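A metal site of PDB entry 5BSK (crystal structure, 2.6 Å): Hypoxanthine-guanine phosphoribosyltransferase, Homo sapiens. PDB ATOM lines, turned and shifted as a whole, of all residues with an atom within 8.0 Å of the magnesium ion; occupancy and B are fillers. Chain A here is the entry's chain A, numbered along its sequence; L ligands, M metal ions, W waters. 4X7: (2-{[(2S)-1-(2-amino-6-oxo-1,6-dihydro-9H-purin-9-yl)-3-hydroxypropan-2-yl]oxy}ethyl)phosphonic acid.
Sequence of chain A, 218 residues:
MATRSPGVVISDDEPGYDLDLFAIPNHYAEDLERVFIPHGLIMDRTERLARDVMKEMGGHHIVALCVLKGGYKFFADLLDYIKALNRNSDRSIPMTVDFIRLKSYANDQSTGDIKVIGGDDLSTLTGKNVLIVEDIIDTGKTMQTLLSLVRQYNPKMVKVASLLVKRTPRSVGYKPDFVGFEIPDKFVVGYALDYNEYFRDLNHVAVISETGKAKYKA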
ATOM      1  N   CYS A  66      20.445   5.015  14.750  1.00  0.00           N
ATOM      2  CA  CYS A  66      21.555   4.865  15.679  1.00  0.00           C
ATOM      3  C   CYS A  66      22.567   3.864  15.140  1.00  0.00           C
ATOM      4  O   CYS A  66      22.205   2.733  14.802  1.00  0.00           O
ATOM      5  CB  CYS A  66      21.064   4.435  17.059  1.00  0.00           C
ATOM      6  SG  CYS A  66      22.388   4.111  18.245  1.00  0.00           S
ATOM      7  N   VAL A  67      23.831   4.273  15.059  1.00  0.00           N
ATOM      8  CA  VAL A  67      24.880   3.396  14.567  1.00  0.00           C
ATOM      9  C   VAL A  67      25.352   2.453  15.659  1.00  0.00           C
ATOM     10  O   VAL A  67      25.632   2.877  16.785  1.00  0.00           O
ATOM     11  CB  VAL A  67      26.079   4.206  14.036  1.00  0.00           C
ATOM     12  CG1 VAL A  67      27.060   3.290  13.331  1.00  0.00           C
ATOM     13  CG2 VAL A  67      25.606   5.310  13.106  1.00  0.00           C
ATOM     14  N   LEU A  68      25.428   1.172  15.333  1.00  0.00           N
ATOM     15  CA  LEU A  68      25.850   0.153  16.292  1.00  0.00           C
ATOM     16  C   LEU A  68      27.198  -0.455  15.887  1.00  0.00           C
ATOM     17  O   LEU A  68      27.470  -0.609  14.687  1.00  0.00           O
ATOM     18  CB  LEU A  68      24.787  -0.937  16.421  1.00  0.00           C
ATOM     19  CG  LEU A  68      23.516  -0.517  17.175  1.00  0.00           C
ATOM     20  CD1 LEU A  68      22.526  -1.668  17.252  1.00  0.00           C
ATOM     21  CD2 LEU A  68      23.865  -0.008  18.559  1.00  0.00           C
ATOM     22  N   LYS A  69      28.025  -0.793  16.860  1.00  0.00           N
ATOM     23  CA  LYS A  69      27.696  -0.648  18.273  1.00  0.00           C
ATOM     24  C   LYS A  69      28.610   0.349  18.970  1.00  0.00           C
ATOM     25  O   LYS A  69      29.737   0.596  18.528  1.00  0.00           O
ATOM     26  CB  LYS A  69      27.742  -1.990  18.972  1.00  0.00           C
ATOM     27  N   GLY A  70      28.123   0.911  20.068  1.00  0.00           N
ATOM     28  CA  GLY A  70      28.867   1.908  20.815  1.00  0.00           C
ATOM     29  C   GLY A  70      28.264   3.287  20.646  1.00  0.00           C
ATOM     30  O   GLY A  70      28.204   3.811  19.541  1.00  0.00           O
ATOM     31  N   GLY A  71      27.802   3.864  21.755  1.00  0.00           N
ATOM     32  CA  GLY A  71      27.237   5.201  21.724  1.00  0.00           C
ATOM     33  C   GLY A  71      25.721   5.220  21.653  1.00  0.00           C
ATOM     34  O   GLY A  71      25.144   6.058  20.954  1.00  0.00           O
ATOM     35  N   TYR A  72      25.092   4.302  22.362  1.00  0.00           N
ATOM     36  CA  TYR A  72      23.632   4.276  22.429  1.00  0.00           C
ATOM     37  C   TYR A  72      23.123   5.316  23.409  1.00  0.00           C
ATOM     38  O   TYR A  72      22.021   5.843  23.254  1.00  0.00           O
ATOM     39  CB  TYR A  72      23.130   2.881  22.819  1.00  0.00           C
ATOM     40  CG  TYR A  72      21.646   2.833  23.075  1.00  0.00           C
ATOM     41  CD1 TYR A  72      20.737   3.170  22.084  1.00  0.00           C
ATOM     42  CD2 TYR A  72      21.141   2.449  24.319  1.00  0.00           C
ATOM     43  CE1 TYR A  72      19.371   3.128  22.303  1.00  0.00           C
ATOM     44  CE2 TYR A  72      19.782   2.411  24.554  1.00  0.00           C
ATOM     45  CZ  TYR A  72      18.903   2.752  23.543  1.00  0.00           C
ATOM     46  OH  TYR A  72      17.546   2.698  23.774  1.00  0.00           O
ATOM     47  N   VAL A 133      22.919   9.211  13.762  1.00  0.00           N
ATOM     48  CA  VAL A 133      23.493   9.623  15.036  1.00  0.00           C
ATOM     49  C   VAL A 133      24.670   8.749  15.430  1.00  0.00           C
ATOM     50  O   VAL A 133      24.545   7.531  15.547  1.00  0.00           O
ATOM     51  CB  VAL A 133      22.436   9.584  16.164  1.00  0.00           C
ATOM     52  CG1 VAL A 133      23.050   9.989  17.482  1.00  0.00           C
ATOM     53  CG2 VAL A 133      21.263  10.487  15.812  1.00  0.00           C
ATOM     54  N   GLU A 134      25.831   9.381  15.620  1.00  0.00           N
ATOM     55  CA  GLU A 134      27.042   8.677  15.998  1.00  0.00           C
ATOM     56  C   GLU A 134      27.630   9.289  17.269  1.00  0.00           C
ATOM     57  O   GLU A 134      27.464  10.477  17.522  1.00  0.00           O
ATOM     58  CB  GLU A 134      28.076   8.725  14.863  1.00  0.00           C
ATOM     59  CG  GLU A 134      29.347   7.948  15.122  1.00  0.00           C
ATOM     60  CD  GLU A 134      29.170   6.448  14.965  1.00  0.00           C
ATOM     61  OE1 GLU A 134      28.839   6.000  13.853  1.00  0.00           O
ATOM     62  OE2 GLU A 134      29.357   5.724  15.964  1.00  0.00           O
ATOM     63  N   ASP A 135      28.308   8.470  18.069  1.00  0.00           N
ATOM     64  CA  ASP A 135      28.923   8.951  19.301  1.00  0.00           C
ATOM     65  C   ASP A 135      30.237   9.657  19.029  1.00  0.00           C
ATOM     66  O   ASP A 135      30.451  10.791  19.483  1.00  0.00           O
ATOM     67  CB  ASP A 135      29.140   7.789  20.274  1.00  0.00           C
ATOM     68  CG  ASP A 135      29.733   6.564  19.606  1.00  0.00           C
ATOM     69  OD1 ASP A 135      29.856   6.569  18.358  1.00  0.00           O
ATOM     70  OD2 ASP A 135      30.054   5.590  20.318  1.00  0.00           O
ATOM     71  N   ILE A 136      31.127   9.012  18.279  1.00  0.00           N
ATOM     72  CA  ILE A 136      32.421   9.589  17.973  1.00  0.00           C
ATOM     73  C   ILE A 136      32.860   9.283  16.541  1.00  0.00           C
ATOM     74  O   ILE A 136      32.618   8.192  16.022  1.00  0.00           O
ATOM     75  CB  ILE A 136      33.506   9.104  18.973  1.00  0.00           C
ATOM     76  CG1 ILE A 136      34.831   9.846  18.744  1.00  0.00           C
ATOM     77  CG2 ILE A 136      33.700   7.594  18.874  1.00  0.00           C
ATOM     78  CD1 ILE A 136      35.929   9.443  19.702  1.00  0.00           C
ATOM     79  N   ILE A 137      33.480  10.264  15.902  1.00  0.00           N
ATOM     80  CA  ILE A 137      34.081  10.070  14.586  1.00  0.00           C
ATOM     81  C   ILE A 137      35.575  10.355  14.672  1.00  0.00           C
ATOM     82  O   ILE A 137      35.997  11.491  14.920  1.00  0.00           O
ATOM     83  CB  ILE A 137      33.438  10.975  13.523  1.00  0.00           C
ATOM     84  CG1 ILE A 137      31.998  10.537  13.257  1.00  0.00           C
ATOM     85  CG2 ILE A 137      34.245  10.940  12.239  1.00  0.00           C
ATOM     86  CD1 ILE A 137      31.337  11.243  12.089  1.00  0.00           C
ATOM     87  N   THR A 142      34.146   5.016   8.965  1.00  0.00           N
ATOM     88  CA  THR A 142      32.873   4.395   9.306  1.00  0.00           C
ATOM     89  C   THR A 142      31.700   5.169   8.713  1.00  0.00           C
ATOM     90  O   THR A 142      30.823   4.596   8.057  1.00  0.00           O
ATOM     91  CB  THR A 142      32.674   4.299  10.829  1.00  0.00           C
ATOM     92  OG1 THR A 142      33.721   3.509  11.407  1.00  0.00           O
ATOM     93  CG2 THR A 142      31.335   3.662  11.157  1.00  0.00           C
ATOM     94  N   MET A 143      31.695   6.479   8.932  1.00  0.00           N
ATOM     95  CA  MET A 143      30.608   7.325   8.458  1.00  0.00           C
ATOM     96  C   MET A 143      30.617   7.478   6.945  1.00  0.00           C
ATOM     97  O   MET A 143      29.565   7.611   6.325  1.00  0.00           O
ATOM     98  CB  MET A 143      30.677   8.708   9.127  1.00  0.00           C
ATOM     99  CG  MET A 143      29.397   9.508   8.996  1.00  0.00           C
ATOM    100  SD  MET A 143      27.970   8.638   9.642  1.00  0.00           S
ATOM    101  CE  MET A 143      28.512   8.289  11.307  1.00  0.00           C
ATOM    102  N   SER A 162      27.080  13.978  15.217  1.00  0.00           N
ATOM    103  CA  SER A 162      28.061  13.267  16.038  1.00  0.00           C
ATOM    104  C   SER A 162      28.398  14.060  17.297  1.00  0.00           C
ATOM    105  O   SER A 162      28.602  15.267  17.253  1.00  0.00           O
ATOM    106  CB  SER A 162      29.332  12.988  15.233  1.00  0.00           C
ATOM    107  OG  SER A 162      30.254  12.236  15.992  1.00  0.00           O
ATOM    108  N   ALA A 192      29.184   7.463  26.580  1.00  0.00           N
ATOM    109  CA  ALA A 192      28.660   6.574  25.546  1.00  0.00           C
ATOM    110  C   ALA A 192      29.740   5.669  24.985  1.00  0.00           C
ATOM    111  O   ALA A 192      29.448   4.722  24.246  1.00  0.00           O
ATOM    112  CB  ALA A 192      28.026   7.384  24.428  1.00  0.00           C
ATOM    113  N   LEU A 193      30.994   5.941  25.339  1.00  0.00           N
ATOM    114  CA  LEU A 193      32.118   5.166  24.827  1.00  0.00           C
ATOM    115  C   LEU A 193      32.643   4.182  25.870  1.00  0.00           C
ATOM    116  O   LEU A 193      32.929   4.570  27.004  1.00  0.00           O
ATOM    117  CB  LEU A 193      33.236   6.096  24.366  1.00  0.00           C
ATOM    118  CG  LEU A 193      32.865   7.051  23.223  1.00  0.00           C
ATOM    119  CD1 LEU A 193      34.039   7.933  22.850  1.00  0.00           C
ATOM    120  CD2 LEU A 193      32.392   6.252  22.015  1.00  0.00           C
HETATM  121  C4  4X7 L   1      37.224   4.889  19.657  1.00  0.00           C
HETATM  122  C5  4X7 L   1      37.904   6.095  19.858  1.00  0.00           C
HETATM  123  C6  4X7 L   1      37.993   6.616  21.131  1.00  0.00           C
HETATM  124  C8  4X7 L   1      37.963   5.577  17.668  1.00  0.00           C
HETATM  125  N1  4X7 L   1      37.407   5.925  22.146  1.00  0.00           N
HETATM  126  N2  4X7 L   1      36.147   4.061  23.038  1.00  0.00           N
HETATM  127  N3  4X7 L   1      36.643   4.229  20.764  1.00  0.00           N
HETATM  128  OAE 4X7 L   1      37.533   6.004  12.951  1.00  0.00           O
HETATM  129  PAV 4X7 L   1      36.073   5.990  12.724  1.00  0.00           P
HETATM  130  OAF 4X7 L   1      35.724   4.818  11.787  1.00  0.00           O
HETATM  131  OAC 4X7 L   1      35.653   7.271  12.090  1.00  0.00           O
HETATM  132  CAJ 4X7 L   1      35.190   5.797  14.320  1.00  0.00           C
HETATM  133  CAI 4X7 L   1      35.856   4.759  15.186  1.00  0.00           C
HETATM  134  OAO 4X7 L   1      35.099   4.622  16.387  1.00  0.00           O
HETATM  135  CAT 4X7 L   1      35.283   3.531  17.199  1.00  0.00           C
HETATM  136  CAH 4X7 L   1      34.321   3.648  18.362  1.00  0.00           C
HETATM  137  OAD 4X7 L   1      32.989   3.883  18.060  1.00  0.00           O
HETATM  138  CAK 4X7 L   1      36.714   3.450  17.644  1.00  0.00           C
HETATM  139  N9  4X7 L   1      37.280   4.606  18.284  1.00  0.00           N
HETATM  140  C2  4X7 L   1      36.735   4.728  21.933  1.00  0.00           C
HETATM  141  O6  4X7 L   1      38.649   7.793  21.369  1.00  0.00           O
HETATM  142  N7  4X7 L   1      38.354   6.504  18.616  1.00  0.00           N
HETATM  143 MG    MG M   1      29.625   4.533  17.626  1.00  0.00          MG
HETATM  144  O   HOH W   1      31.464   5.222  16.804  1.00  0.00           O
HETATM  145  O   HOH W   2      31.050   3.700  19.207  1.00  0.00           O
HETATM  146  O   HOH W   3      30.130   3.442  15.921  1.00  0.00           O
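The backbone NH (N) of Thr 142 sits close to an oxygen (OAF) of the ligand.
OG1 of Thr 142 is in hydrogen-bond range of OAF of the ligand (2.4 Å).
OD2 of Asp 135 sits close to N of Gly 71, 3.2 Å away.
Within 4 Å of the magnesium ion: Gly 70, Glu 134 and Asp 135.
Along chain A the residues within 4 Å of the magnesium ion span positions 70 to 135.
The nearest printed residue that does not touch the magnesium ion is Lys 69 (4.04 Å).
The magnesium ion is bound by OE2 of Glu 134 (2.1 Å), water W3 (2.1 Å), water W1 (2.1 Å), OD1 of Asp 135 (2.2 Å), water W2 (2.3 Å) and O of Gly 70 (2.5 Å).
The magnesium ion has six donor atoms within binding distance.
Water W2 bridges the side-chain carboxylate (OD2) of Asp 135 (2.4 Å) and the backbone carbonyl oxygen (O) of Lys 69 (3.4 Å).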
